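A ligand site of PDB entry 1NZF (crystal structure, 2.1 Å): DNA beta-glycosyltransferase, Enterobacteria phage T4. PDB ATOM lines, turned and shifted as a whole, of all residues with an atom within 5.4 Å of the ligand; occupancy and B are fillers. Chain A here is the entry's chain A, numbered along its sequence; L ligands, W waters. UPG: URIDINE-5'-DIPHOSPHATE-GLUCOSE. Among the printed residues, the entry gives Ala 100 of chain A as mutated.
Residues that only touch the ligand: Val 18 (3.3 Å), Gly 187 (3.6 Å), Gly 188 (3.2 Å), Phe 213 (3.3 Å), Gly 236 (3.98 Å), Lys 237 (3.3 Å), Pro 239 (3.96 Å), Val 243 (3.7 Å), Phe 265 (3.8 Å) and Thr 267 (3.7 Å). Hydrophobic or aromatic side chains within 4 Å of the ligand: Val 18, Phe 213, Ile 238, Met 240, Val 243, Tyr 261, Phe 265 and Leu 268. 23 residues have an atom within 4 Å of the ligand: Val 18, Glu 22, Thr 99, Gln 137, Gly 187, Gly 188, Ser 189, Arg 191, Arg 195, Phe 213, Gly 214, Gly 236, Lys 237, Ile 238, Pro 239, Met 240, Val 243, Tyr 261, Phe 265, Thr 267, Leu 268, Arg 269 and Glu 272. The nearest printed residue that does not touch the ligand is Glu 163 (4.1 Å).
The side-chain hydroxyl (OG1) of Thr 99 is in hydrogen-bond range of the side-chain carboxylate (OE2) of Glu 22 (2.7 Å). The side-chain hydroxyl (OH) of Tyr 165 sits at hydrogen-bond distance from the side-chain carboxylate (OE1) of Glu 22 (2.7 Å). OE2 of Glu 272 is in salt-bridge range of NZ of Lys 166, at 2.6 Å. The guanidinium group (NH1) of Arg 269 is in hydrogen-bond range of the backbone carbonyl oxygen (O) of Gly 187 (2.8 Å). The guanidinium group of Arg 269 sits at hydrogen-bond distance from the side-chain hydroxyl of Tyr 186 (3.4 Å). NE2 of Gln 137 lies within hydrogen-bond range of O of Ile 266 (2.9 Å). The backbone carbonyl oxygen (O) of Met 240 sits at hydrogen-bond distance from the side-chain amino group (NZ) of Lys 166. The backbone carbonyl oxygen (O) of Phe 15 lies within hydrogen-bond range of the backbone NH (N) of Met 240.
The backbone carbonyl oxygen (O) of Thr 99 is in hydrogen-bond range of an oxygen (O3') of the ligand. OE1 of Glu 22 lies within hydrogen-bond range of O6' of the ligand (2.6 Å). OE2 of Glu 272 sits at hydrogen-bond distance from O2C of the ligand. NH2 of Arg 269 lies within salt-bridge range of O2B of the ligand, 2.8 Å away. The backbone NH (N) of Ile 238 sits at hydrogen-bond distance from an oxygen (O4) of the ligand (2.8 Å). N3 of the ligand is in hydrogen-bond range of O of Ile 238. NH2 of Arg 191 lies within salt-bridge range of O1B of the ligand (2.8 Å). OH of Tyr 261 is in hydrogen-bond range of O2' of the ligand, at 2.9 Å. O1B of the ligand is in salt-bridge range of NH1 of Arg 195 (2.9 Å). The backbone NH of Ser 189 is in hydrogen-bond range of an oxygen (O1A) of the ligand (3.0 Å). OG of Ser 189 lies within hydrogen-bond range of O2A of the ligand, 3.2 Å away. N of Leu 268 is in hydrogen-bond range of O4' of the ligand, 3.1 Å away. The side-chain amide nitrogen (NE2) of Gln 137 is in hydrogen-bond range of an oxygen (O3') of the ligand. N of Met 240 lies close to O2 of the ligand (3.4 Å). N of Gly 214 sits close to O4 of the ligand (3.4 Å).
Water W9 lies within hydrogen-bond range of an oxygen (O2A) of the ligand and the side-chain hydroxyl of Ser 189. Water W1 lies within hydrogen-bond range of O1B of the ligand (2.8 Å), NH2 of Arg 195 (2.9 Å) and NH1 of Arg 191 (3.1 Å). Water W6 lies within hydrogen-bond range of O2B of the ligand (2.8 Å) and N of Arg 269 (2.9 Å). Water W3 lies within hydrogen-bond range of OE1 of Gln 137 (2.7 Å), OE1 of Glu 22 (2.8 Å) and O4' of the ligand (2.8 Å). Water W4 bridges an oxygen (O2A) of the ligand (2.9 Å) and the side-chain hydroxyl (OG) of Ser 189 (2.9 Å). Water W10 lies within hydrogen-bond range of O2 of the ligand (3.2 Å), O of Phe 15 (3.3 Å) and N of Val 18 (3.4 Å).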
ATOM      1  N   PHE A  15      31.153 -18.294  17.560  1.00  0.00           N
ATOM      2  CA  PHE A  15      30.863 -16.862  17.545  1.00  0.00           C
ATOM      3  C   PHE A  15      29.396 -16.473  17.415  1.00  0.00           C
ATOM      4  O   PHE A  15      29.077 -15.317  17.129  1.00  0.00           O
ATOM      5  CB  PHE A  15      31.672 -16.192  16.433  1.00  0.00           C
ATOM      6  CG  PHE A  15      33.140 -16.496  16.503  1.00  0.00           C
ATOM      7  CD1 PHE A  15      33.700 -17.489  15.721  1.00  0.00           C
ATOM      8  CD2 PHE A  15      33.952 -15.818  17.415  1.00  0.00           C
ATOM      9  CE1 PHE A  15      35.044 -17.821  15.841  1.00  0.00           C
ATOM     10  CE2 PHE A  15      35.302 -16.139  17.547  1.00  0.00           C
ATOM     11  CZ  PHE A  15      35.853 -17.141  16.762  1.00  0.00           C
ATOM     12  N   VAL A  18      27.781 -13.242  21.858  1.00  0.00           N
ATOM     13  CA  VAL A  18      28.821 -12.338  22.316  1.00  0.00           C
ATOM     14  C   VAL A  18      29.667 -12.884  23.478  1.00  0.00           C
ATOM     15  O   VAL A  18      30.895 -12.759  23.469  1.00  0.00           O
ATOM     16  CB  VAL A  18      28.214 -10.954  22.692  1.00  0.00           C
ATOM     17  CG1 VAL A  18      29.277 -10.031  23.246  1.00  0.00           C
ATOM     18  CG2 VAL A  18      27.576 -10.325  21.452  1.00  0.00           C
ATOM     19  N   GLU A  22      33.698 -13.488  23.017  1.00  0.00           N
ATOM     20  CA  GLU A  22      34.682 -12.793  23.847  1.00  0.00           C
ATOM     21  C   GLU A  22      35.591 -13.793  24.556  1.00  0.00           C
ATOM     22  O   GLU A  22      36.793 -13.564  24.694  1.00  0.00           O
ATOM     23  CB  GLU A  22      33.985 -11.884  24.862  1.00  0.00           C
ATOM     24  CG  GLU A  22      34.926 -11.212  25.855  1.00  0.00           C
ATOM     25  CD  GLU A  22      34.358  -9.911  26.419  1.00  0.00           C
ATOM     26  OE1 GLU A  22      34.458  -8.874  25.732  1.00  0.00           O
ATOM     27  OE2 GLU A  22      33.806  -9.945  27.536  1.00  0.00           O
ATOM     28  N   THR A  99      34.476  -6.921  32.016  1.00  0.00           N
ATOM     29  CA  THR A  99      34.311  -6.208  30.750  1.00  0.00           C
ATOM     30  C   THR A  99      32.997  -5.437  30.592  1.00  0.00           C
ATOM     31  O   THR A  99      32.842  -4.652  29.650  1.00  0.00           O
ATOM     32  CB  THR A  99      34.490  -7.164  29.533  1.00  0.00           C
ATOM     33  OG1 THR A  99      33.389  -8.062  29.446  1.00  0.00           O
ATOM     34  CG2 THR A  99      35.778  -7.954  29.672  1.00  0.00           C
ATOM     35  N   ALA A 100      32.044  -5.677  31.491  1.00  0.00           N
ATOM     36  CA  ALA A 100      30.758  -4.986  31.451  1.00  0.00           C
ATOM     37  C   ALA A 100      30.375  -4.587  32.871  1.00  0.00           C
ATOM     38  O   ALA A 100      30.326  -5.430  33.767  1.00  0.00           O
ATOM     39  CB  ALA A 100      29.676  -5.873  30.847  1.00  0.00           C
ATOM     40  N   ARG A 102      27.629  -3.959  34.403  1.00  0.00           N
ATOM     41  CA  ARG A 102      26.522  -4.661  35.032  1.00  0.00           C
ATOM     42  C   ARG A 102      26.813  -6.103  35.449  1.00  0.00           C
ATOM     43  O   ARG A 102      25.945  -6.764  36.022  1.00  0.00           O
ATOM     44  CB  ARG A 102      25.310  -4.668  34.091  1.00  0.00           C
ATOM     45  CG  ARG A 102      25.423  -5.657  32.941  1.00  0.00           C
ATOM     46  CD  ARG A 102      24.246  -5.578  31.988  1.00  0.00           C
ATOM     47  NE  ARG A 102      24.321  -6.600  30.938  1.00  0.00           N
ATOM     48  CZ  ARG A 102      25.231  -6.617  29.969  1.00  0.00           C
ATOM     49  NH1 ARG A 102      26.145  -5.663  29.895  1.00  0.00           N
ATOM     50  NH2 ARG A 102      25.242  -7.608  29.085  1.00  0.00           N
ATOM     51  N   GLN A 137      38.190  -3.351  32.872  1.00  0.00           N
ATOM     52  CA  GLN A 137      38.427  -2.814  31.541  1.00  0.00           C
ATOM     53  C   GLN A 137      38.379  -1.288  31.639  1.00  0.00           C
ATOM     54  O   GLN A 137      38.955  -0.568  30.824  1.00  0.00           O
ATOM     55  CB  GLN A 137      37.338  -3.328  30.585  1.00  0.00           C
ATOM     56  CG  GLN A 137      37.500  -2.918  29.133  1.00  0.00           C
ATOM     57  CD  GLN A 137      36.553  -3.688  28.234  1.00  0.00           C
ATOM     58  OE1 GLN A 137      36.568  -4.921  28.232  1.00  0.00           O
ATOM     59  NE2 GLN A 137      35.741  -2.975  27.457  1.00  0.00           N
ATOM     60  N   GLU A 163      39.541  -5.057  26.030  1.00  0.00           N
ATOM     61  CA  GLU A 163      38.890  -4.994  24.725  1.00  0.00           C
ATOM     62  C   GLU A 163      39.758  -4.901  23.461  1.00  0.00           C
ATOM     63  O   GLU A 163      39.228  -4.942  22.353  1.00  0.00           O
ATOM     64  CB  GLU A 163      37.852  -3.864  24.723  1.00  0.00           C
ATOM     65  CG  GLU A 163      38.328  -2.471  24.358  1.00  0.00           C
ATOM     66  CD  GLU A 163      39.469  -1.956  25.226  1.00  0.00           C
ATOM     67  OE1 GLU A 163      39.494  -2.208  26.442  1.00  0.00           O
ATOM     68  OE2 GLU A 163      40.339  -1.251  24.679  1.00  0.00           O
ATOM     69  N   TYR A 165      41.625  -7.122  22.441  1.00  0.00           N
ATOM     70  CA  TYR A 165      41.890  -8.481  21.975  1.00  0.00           C
ATOM     71  C   TYR A 165      41.723  -8.724  20.479  1.00  0.00           C
ATOM     72  O   TYR A 165      42.447  -9.530  19.900  1.00  0.00           O
ATOM     73  CB  TYR A 165      41.080  -9.516  22.789  1.00  0.00           C
ATOM     74  CG  TYR A 165      39.575  -9.339  22.872  1.00  0.00           C
ATOM     75  CD1 TYR A 165      38.755  -9.514  21.749  1.00  0.00           C
ATOM     76  CD2 TYR A 165      38.960  -9.105  24.098  1.00  0.00           C
ATOM     77  CE1 TYR A 165      37.359  -9.471  21.862  1.00  0.00           C
ATOM     78  CE2 TYR A 165      37.570  -9.061  24.224  1.00  0.00           C
ATOM     79  CZ  TYR A 165      36.780  -9.250  23.106  1.00  0.00           C
ATOM     80  OH  TYR A 165      35.416  -9.207  23.244  1.00  0.00           O
ATOM     81  N   LYS A 166      40.806  -8.020  19.834  1.00  0.00           N
ATOM     82  CA  LYS A 166      40.627  -8.202  18.398  1.00  0.00           C
ATOM     83  C   LYS A 166      41.756  -7.591  17.563  1.00  0.00           C
ATOM     84  O   LYS A 166      42.212  -8.197  16.593  1.00  0.00           O
ATOM     85  CB  LYS A 166      39.290  -7.622  17.923  1.00  0.00           C
ATOM     86  CG  LYS A 166      38.131  -8.606  17.971  1.00  0.00           C
ATOM     87  CD  LYS A 166      36.944  -8.063  17.214  1.00  0.00           C
ATOM     88  CE  LYS A 166      35.795  -9.058  17.191  1.00  0.00           C
ATOM     89  NZ  LYS A 166      34.622  -8.514  16.451  1.00  0.00           N
ATOM     90  N   TYR A 186      24.986   0.850  13.306  1.00  0.00           N
ATOM     91  CA  TYR A 186      25.319   0.567  14.688  1.00  0.00           C
ATOM     92  C   TYR A 186      24.899  -0.882  14.922  1.00  0.00           C
ATOM     93  O   TYR A 186      23.783  -1.269  14.597  1.00  0.00           O
ATOM     94  CB  TYR A 186      24.547   1.469  15.649  1.00  0.00           C
ATOM     95  CG  TYR A 186      24.903   1.265  17.115  1.00  0.00           C
ATOM     96  CD1 TYR A 186      25.992   1.922  17.688  1.00  0.00           C
ATOM     97  CD2 TYR A 186      24.130   0.429  17.930  1.00  0.00           C
ATOM     98  CE1 TYR A 186      26.318   1.757  19.033  1.00  0.00           C
ATOM     99  CE2 TYR A 186      24.451   0.255  19.286  1.00  0.00           C
ATOM    100  CZ  TYR A 186      25.542   0.929  19.834  1.00  0.00           C
ATOM    101  OH  TYR A 186      25.826   0.790  21.178  1.00  0.00           O
ATOM    102  N   GLY A 187      25.818  -1.682  15.453  1.00  0.00           N
ATOM    103  CA  GLY A 187      25.510  -3.082  15.716  1.00  0.00           C
ATOM    104  C   GLY A 187      25.656  -3.368  17.193  1.00  0.00           C
ATOM    105  O   GLY A 187      26.749  -3.285  17.733  1.00  0.00           O
ATOM    106  N   GLY A 188      24.546  -3.711  17.841  1.00  0.00           N
ATOM    107  CA  GLY A 188      24.609  -3.994  19.258  1.00  0.00           C
ATOM    108  C   GLY A 188      23.282  -4.394  19.864  1.00  0.00           C
ATOM    109  O   GLY A 188      22.355  -4.797  19.149  1.00  0.00           O
ATOM    110  N   SER A 189      23.191  -4.272  21.179  1.00  0.00           N
ATOM    111  CA  SER A 189      21.989  -4.644  21.902  1.00  0.00           C
ATOM    112  C   SER A 189      21.374  -3.434  22.575  1.00  0.00           C
ATOM    113  O   SER A 189      22.009  -2.393  22.715  1.00  0.00           O
ATOM    114  CB  SER A 189      22.323  -5.691  22.964  1.00  0.00           C
ATOM    115  OG  SER A 189      22.941  -6.828  22.391  1.00  0.00           O
ATOM    116  N   ARG A 191      19.859  -1.358  25.748  1.00  0.00           N
ATOM    117  CA  ARG A 191      20.179  -1.229  27.156  1.00  0.00           C
ATOM    118  C   ARG A 191      19.437   0.014  27.632  1.00  0.00           C
ATOM    119  O   ARG A 191      19.589   1.078  27.051  1.00  0.00           O
ATOM    120  CB  ARG A 191      21.686  -1.063  27.365  1.00  0.00           C
ATOM    121  CG  ARG A 191      22.119  -1.167  28.824  1.00  0.00           C
ATOM    122  CD  ARG A 191      23.627  -0.918  28.972  1.00  0.00           C
ATOM    123  NE  ARG A 191      24.412  -1.896  28.232  1.00  0.00           N
ATOM    124  CZ  ARG A 191      25.700  -1.766  27.927  1.00  0.00           C
ATOM    125  NH1 ARG A 191      26.374  -0.688  28.323  1.00  0.00           N
ATOM    126  NH2 ARG A 191      26.311  -2.714  27.236  1.00  0.00           N
ATOM    127  N   ARG A 195      22.110   4.715  27.560  1.00  0.00           N
ATOM    128  CA  ARG A 195      22.369   4.085  26.273  1.00  0.00           C
ATOM    129  C   ARG A 195      21.109   4.166  25.405  1.00  0.00           C
ATOM    130  O   ARG A 195      21.183   4.543  24.232  1.00  0.00           O
ATOM    131  CB  ARG A 195      22.805   2.626  26.470  1.00  0.00           C
ATOM    132  CG  ARG A 195      23.087   1.839  25.178  1.00  0.00           C
ATOM    133  CD  ARG A 195      24.066   2.559  24.233  1.00  0.00           C
ATOM    134  NE  ARG A 195      25.392   2.778  24.818  1.00  0.00           N
ATOM    135  CZ  ARG A 195      26.280   1.821  25.053  1.00  0.00           C
ATOM    136  NH1 ARG A 195      26.010   0.547  24.754  1.00  0.00           N
ATOM    137  NH2 ARG A 195      27.454   2.127  25.598  1.00  0.00           N
ATOM    138  N   PHE A 213      21.942  -3.262  13.443  1.00  0.00           N
ATOM    139  CA  PHE A 213      22.002  -4.725  13.450  1.00  0.00           C
ATOM    140  C   PHE A 213      22.244  -5.215  14.875  1.00  0.00           C
ATOM    141  O   PHE A 213      22.592  -4.425  15.758  1.00  0.00           O
ATOM    142  CB  PHE A 213      23.047  -5.283  12.456  1.00  0.00           C
ATOM    143  CG  PHE A 213      24.496  -4.943  12.772  1.00  0.00           C
ATOM    144  CD1 PHE A 213      25.033  -3.720  12.411  1.00  0.00           C
ATOM    145  CD2 PHE A 213      25.335  -5.899  13.353  1.00  0.00           C
ATOM    146  CE1 PHE A 213      26.392  -3.445  12.600  1.00  0.00           C
ATOM    147  CE2 PHE A 213      26.698  -5.632  13.555  1.00  0.00           C
ATOM    148  CZ  PHE A 213      27.231  -4.401  13.180  1.00  0.00           C
ATOM    149  N   GLY A 214      22.049  -6.512  15.103  1.00  0.00           N
ATOM    150  CA  GLY A 214      22.219  -7.075  16.432  1.00  0.00           C
ATOM    151  C   GLY A 214      20.871  -7.593  16.896  1.00  0.00           C
ATOM    152  O   GLY A 214      19.910  -7.559  16.137  1.00  0.00           O
ATOM    153  N   ASN A 215      20.777  -8.059  18.144  1.00  0.00           N
ATOM    154  CA  ASN A 215      19.506  -8.584  18.632  1.00  0.00           C
ATOM    155  C   ASN A 215      18.541  -7.521  19.131  1.00  0.00           C
ATOM    156  O   ASN A 215      17.433  -7.839  19.586  1.00  0.00           O
ATOM    157  CB  ASN A 215      19.748  -9.646  19.722  1.00  0.00           C
ATOM    158  CG  ASN A 215      20.422  -9.089  20.963  1.00  0.00           C
ATOM    159  OD1 ASN A 215      20.838  -9.835  21.848  1.00  0.00           O
ATOM    160  ND2 ASN A 215      20.520  -7.769  21.043  1.00  0.00           N
ATOM    161  N   GLY A 236      18.892  -7.884  12.552  1.00  0.00           N
ATOM    162  CA  GLY A 236      19.256  -9.170  13.150  1.00  0.00           C
ATOM    163  C   GLY A 236      20.697  -9.321  13.590  1.00  0.00           C
ATOM    164  O   GLY A 236      21.594  -8.657  13.075  1.00  0.00           O
ATOM    165  N   LYS A 237      20.917 -10.225  14.540  1.00  0.00           N
ATOM    166  CA  LYS A 237      22.242 -10.488  15.094  1.00  0.00           C
ATOM    167  C   LYS A 237      23.101 -11.320  14.147  1.00  0.00           C
ATOM    168  O   LYS A 237      22.643 -12.300  13.563  1.00  0.00           O
ATOM    169  CB  LYS A 237      22.112 -11.200  16.451  1.00  0.00           C
ATOM    170  CG  LYS A 237      23.441 -11.377  17.201  1.00  0.00           C
ATOM    171  CD  LYS A 237      23.246 -11.887  18.635  1.00  0.00           C
ATOM    172  CE  LYS A 237      22.929 -13.373  18.689  1.00  0.00           C
ATOM    173  NZ  LYS A 237      22.728 -13.865  20.094  1.00  0.00           N
ATOM    174  N   ILE A 238      24.367 -10.932  14.005  1.00  0.00           N
ATOM    175  CA  ILE A 238      25.298 -11.659  13.159  1.00  0.00           C
ATOM    176  C   ILE A 238      26.459 -12.122  14.034  1.00  0.00           C
ATOM    177  O   ILE A 238      26.646 -11.627  15.147  1.00  0.00           O
ATOM    178  CB  ILE A 238      25.861 -10.741  12.046  1.00  0.00           C
ATOM    179  CG1 ILE A 238      26.778  -9.679  12.653  1.00  0.00           C
ATOM    180  CG2 ILE A 238      24.716 -10.060  11.292  1.00  0.00           C
ATOM    181  CD1 ILE A 238      27.496  -8.843  11.624  1.00  0.00           C
ATOM    182  N   PRO A 239      27.256 -13.098  13.555  1.00  0.00           N
ATOM    183  CA  PRO A 239      28.389 -13.613  14.316  1.00  0.00           C
ATOM    184  C   PRO A 239      29.322 -12.451  14.689  1.00  0.00           C
ATOM    185  O   PRO A 239      29.491 -11.518  13.907  1.00  0.00           O
ATOM    186  CB  PRO A 239      29.047 -14.582  13.350  1.00  0.00           C
ATOM    187  CG  PRO A 239      27.889 -15.105  12.565  1.00  0.00           C
ATOM    188  CD  PRO A 239      27.095 -13.860  12.294  1.00  0.00           C
ATOM    189  N   MET A 240      29.919 -12.523  15.870  1.00  0.00           N
ATOM    190  CA  MET A 240      30.798 -11.438  16.301  1.00  0.00           C
ATOM    191  C   MET A 240      32.058 -11.274  15.443  1.00  0.00           C
ATOM    192  O   MET A 240      32.662 -10.198  15.440  1.00  0.00           O
ATOM    193  CB  MET A 240      31.226 -11.612  17.760  1.00  0.00           C
ATOM    194  CG  MET A 240      31.944 -10.372  18.277  1.00  0.00           C
ATOM    195  SD  MET A 240      33.278 -10.660  19.429  1.00  0.00           S
ATOM    196  CE  MET A 240      32.460 -10.296  20.973  1.00  0.00           C
ATOM    197  N   VAL A 243      31.589  -8.453  12.535  1.00  0.00           N
ATOM    198  CA  VAL A 243      31.123  -7.112  12.882  1.00  0.00           C
ATOM    199  C   VAL A 243      31.781  -5.974  12.080  1.00  0.00           C
ATOM    200  O   VAL A 243      31.080  -5.109  11.568  1.00  0.00           O
ATOM    201  CB  VAL A 243      31.307  -6.850  14.393  1.00  0.00           C
ATOM    202  CG1 VAL A 243      30.979  -5.398  14.725  1.00  0.00           C
ATOM    203  CG2 VAL A 243      30.407  -7.784  15.181  1.00  0.00           C
ATOM    204  N   TYR A 261      30.457   4.331  31.801  1.00  0.00           N
ATOM    205  CA  TYR A 261      31.370   3.904  30.734  1.00  0.00           C
ATOM    206  C   TYR A 261      32.129   5.128  30.228  1.00  0.00           C
ATOM    207  O   TYR A 261      33.313   5.035  29.897  1.00  0.00           O
ATOM    208  CB  TYR A 261      30.609   3.258  29.573  1.00  0.00           C
ATOM    209  CG  TYR A 261      30.286   1.793  29.786  1.00  0.00           C
ATOM    210  CD1 TYR A 261      29.145   1.411  30.495  1.00  0.00           C
ATOM    211  CD2 TYR A 261      31.130   0.799  29.298  1.00  0.00           C
ATOM    212  CE1 TYR A 261      28.847   0.064  30.697  1.00  0.00           C
ATOM    213  CE2 TYR A 261      30.846  -0.551  29.496  1.00  0.00           C
ATOM    214  CZ  TYR A 261      29.702  -0.914  30.188  1.00  0.00           C
ATOM    215  OH  TYR A 261      29.417  -2.242  30.392  1.00  0.00           O
ATOM    216  N   PHE A 265      35.732   3.500  30.283  1.00  0.00           N
ATOM    217  CA  PHE A 265      35.892   2.294  29.473  1.00  0.00           C
ATOM    218  C   PHE A 265      36.110   2.602  28.000  1.00  0.00           C
ATOM    219  O   PHE A 265      35.558   3.565  27.469  1.00  0.00           O
ATOM    220  CB  PHE A 265      34.615   1.444  29.488  1.00  0.00           C
ATOM    221  CG  PHE A 265      34.519   0.442  30.604  1.00  0.00           C
ATOM    222  CD1 PHE A 265      34.403   0.864  31.928  1.00  0.00           C
ATOM    223  CD2 PHE A 265      34.467  -0.921  30.319  1.00  0.00           C
ATOM    224  CE1 PHE A 265      34.223  -0.068  32.949  1.00  0.00           C
ATOM    225  CE2 PHE A 265      34.292  -1.855  31.331  1.00  0.00           C
ATOM    226  CZ  PHE A 265      34.167  -1.432  32.651  1.00  0.00           C
ATOM    227  N   ILE A 266      36.930   1.785  27.355  1.00  0.00           N
ATOM    228  CA  ILE A 266      37.072   1.863  25.914  1.00  0.00           C
ATOM    229  C   ILE A 266      36.363   0.542  25.649  1.00  0.00           C
ATOM    230  O   ILE A 266      36.647  -0.461  26.302  1.00  0.00           O
ATOM    231  CB  ILE A 266      38.529   1.782  25.424  1.00  0.00           C
ATOM    232  CG1 ILE A 266      39.266   3.096  25.747  1.00  0.00           C
ATOM    233  CG2 ILE A 266      38.549   1.552  23.909  1.00  0.00           C
ATOM    234  CD1 ILE A 266      38.617   4.324  25.111  1.00  0.00           C
ATOM    235  N   THR A 267      35.406   0.534  24.733  1.00  0.00           N
ATOM    236  CA  THR A 267      34.647  -0.684  24.427  1.00  0.00           C
ATOM    237  C   THR A 267      35.131  -1.354  23.148  1.00  0.00           C
ATOM    238  O   THR A 267      35.761  -0.724  22.319  1.00  0.00           O
ATOM    239  CB  THR A 267      33.148  -0.361  24.306  1.00  0.00           C
ATOM    240  OG1 THR A 267      32.959   0.669  23.335  1.00  0.00           O
ATOM    241  CG2 THR A 267      32.583   0.106  25.655  1.00  0.00           C
ATOM    242  N   LEU A 268      34.822  -2.643  23.001  1.00  0.00           N
ATOM    243  CA  LEU A 268      35.225  -3.393  21.812  1.00  0.00           C
ATOM    244  C   LEU A 268      34.801  -2.655  20.536  1.00  0.00           C
ATOM    245  O   LEU A 268      35.535  -2.640  19.549  1.00  0.00           O
ATOM    246  CB  LEU A 268      34.599  -4.790  21.833  1.00  0.00           C
ATOM    247  CG  LEU A 268      34.922  -5.690  20.648  1.00  0.00           C
ATOM    248  CD1 LEU A 268      36.432  -5.890  20.550  1.00  0.00           C
ATOM    249  CD2 LEU A 268      34.210  -7.025  20.819  1.00  0.00           C
ATOM    250  N   ARG A 269      33.601  -2.077  20.578  1.00  0.00           N
ATOM    251  CA  ARG A 269      33.007  -1.324  19.479  1.00  0.00           C
ATOM    252  C   ARG A 269      33.989  -0.305  18.889  1.00  0.00           C
ATOM    253  O   ARG A 269      34.079  -0.129  17.672  1.00  0.00           O
ATOM    254  CB  ARG A 269      31.758  -0.616  20.008  1.00  0.00           C
ATOM    255  CG  ARG A 269      31.064   0.324  19.061  1.00  0.00           C
ATOM    256  CD  ARG A 269      29.819   0.900  19.751  1.00  0.00           C
ATOM    257  NE  ARG A 269      29.007  -0.165  20.325  1.00  0.00           N
ATOM    258  CZ  ARG A 269      28.380  -1.098  19.612  1.00  0.00           C
ATOM    259  NH1 ARG A 269      28.462  -1.088  18.290  1.00  0.00           N
ATOM    260  NH2 ARG A 269      27.701  -2.064  20.227  1.00  0.00           N
ATOM    261  N   GLU A 272      36.341  -2.110  16.650  1.00  0.00           N
ATOM    262  CA  GLU A 272      35.626  -2.726  15.536  1.00  0.00           C
ATOM    263  C   GLU A 272      35.244  -1.677  14.508  1.00  0.00           C
ATOM    264  O   GLU A 272      35.202  -1.959  13.309  1.00  0.00           O
ATOM    265  CB  GLU A 272      34.373  -3.447  16.025  1.00  0.00           C
ATOM    266  CG  GLU A 272      34.642  -4.579  16.996  1.00  0.00           C
ATOM    267  CD  GLU A 272      33.378  -5.246  17.493  1.00  0.00           C
ATOM    268  OE1 GLU A 272      32.446  -4.507  17.890  1.00  0.00           O
ATOM    269  OE2 GLU A 272      33.306  -6.489  17.487  1.00  0.00           O
HETATM  270  N1  UPG L   1      27.724  -7.877  18.125  1.00  0.00           N
HETATM  271  C2  UPG L   1      27.638  -9.091  17.463  1.00  0.00           C
HETATM  272  N3  UPG L   1      26.632  -9.184  16.541  1.00  0.00           N
HETATM  273  C4  UPG L   1      25.706  -8.223  16.221  1.00  0.00           C
HETATM  274  C5  UPG L   1      25.837  -6.996  16.957  1.00  0.00           C
HETATM  275  C6  UPG L   1      26.829  -6.872  17.866  1.00  0.00           C
HETATM  276  O2  UPG L   1      28.403 -10.023  17.683  1.00  0.00           O
HETATM  277  O4  UPG L   1      24.814  -8.491  15.406  1.00  0.00           O
HETATM  278  C1C UPG L   1      28.825  -7.730  19.090  1.00  0.00           C
HETATM  279  C2C UPG L   1      29.914  -6.720  18.694  1.00  0.00           C
HETATM  280  O2C UPG L   1      31.157  -7.371  18.763  1.00  0.00           O
HETATM  281  C3C UPG L   1      29.754  -5.642  19.773  1.00  0.00           C
HETATM  282  C4C UPG L   1      29.274  -6.460  20.960  1.00  0.00           C
HETATM  283  O4C UPG L   1      28.318  -7.345  20.346  1.00  0.00           O
HETATM  284  O3C UPG L   1      30.998  -5.014  20.053  1.00  0.00           O
HETATM  285  C5C UPG L   1      28.665  -5.725  22.138  1.00  0.00           C
HETATM  286  O5C UPG L   1      27.630  -4.852  21.730  1.00  0.00           O
HETATM  287  PA  UPG L   1      26.516  -4.371  22.763  1.00  0.00           P
HETATM  288  O1A UPG L   1      25.779  -3.228  22.159  1.00  0.00           O
HETATM  289  O2A UPG L   1      25.770  -5.559  23.246  1.00  0.00           O
HETATM  290  O3A UPG L   1      27.387  -3.828  24.027  1.00  0.00           O
HETATM  291  PB  UPG L   1      28.438  -2.584  24.137  1.00  0.00           P
HETATM  292  O1B UPG L   1      27.910  -1.665  25.171  1.00  0.00           O
HETATM  293  O2B UPG L   1      28.752  -2.071  22.778  1.00  0.00           O
HETATM  294  O3B UPG L   1      29.732  -3.320  24.701  1.00  0.00           O
HETATM  295  C1' UPG L   1      29.716  -4.257  25.774  1.00  0.00           C
HETATM  296  C2' UPG L   1      30.473  -3.776  26.988  1.00  0.00           C
HETATM  297  C3' UPG L   1      31.901  -3.431  26.538  1.00  0.00           C
HETATM  298  C4' UPG L   1      32.550  -4.660  25.907  1.00  0.00           C
HETATM  299  C5' UPG L   1      31.658  -5.252  24.798  1.00  0.00           C
HETATM  300  C6' UPG L   1      32.166  -6.614  24.330  1.00  0.00           C
HETATM  301  O2' UPG L   1      29.831  -2.639  27.540  1.00  0.00           O
HETATM  302  O3' UPG L   1      32.669  -2.985  27.652  1.00  0.00           O
HETATM  303  O4' UPG L   1      33.825  -4.324  25.379  1.00  0.00           O
HETATM  304  O5' UPG L   1      30.305  -5.461  25.278  1.00  0.00           O
HETATM  305  O6' UPG L   1      32.222  -7.528  25.419  1.00  0.00           O
HETATM  306  O   HOH W   1      29.032   0.165  26.968  1.00  0.00           O
HETATM  307  O   HOH W   2      30.014   0.632  23.226  1.00  0.00           O
HETATM  308  O   HOH W   3      35.612  -6.382  26.160  1.00  0.00           O
HETATM  309  O   HOH W   4      25.339  -7.036  20.823  1.00  0.00           O
HETATM  310  O   HOH W   5      24.516  -0.944  22.814  1.00  0.00           O
HETATM  311  O   HOH W   6      31.296  -3.051  22.080  1.00  0.00           O
HETATM  312  O   HOH W   7      27.601  -6.454  27.306  1.00  0.00           O
HETATM  313  O   HOH W   8      25.230  -5.321  26.151  1.00  0.00           O
HETATM  314  O   HOH W   9      25.691  -8.193  23.882  1.00  0.00           O
HETATM  315  O   HOH W  10      27.318 -12.874  18.477  1.00  0.00           O
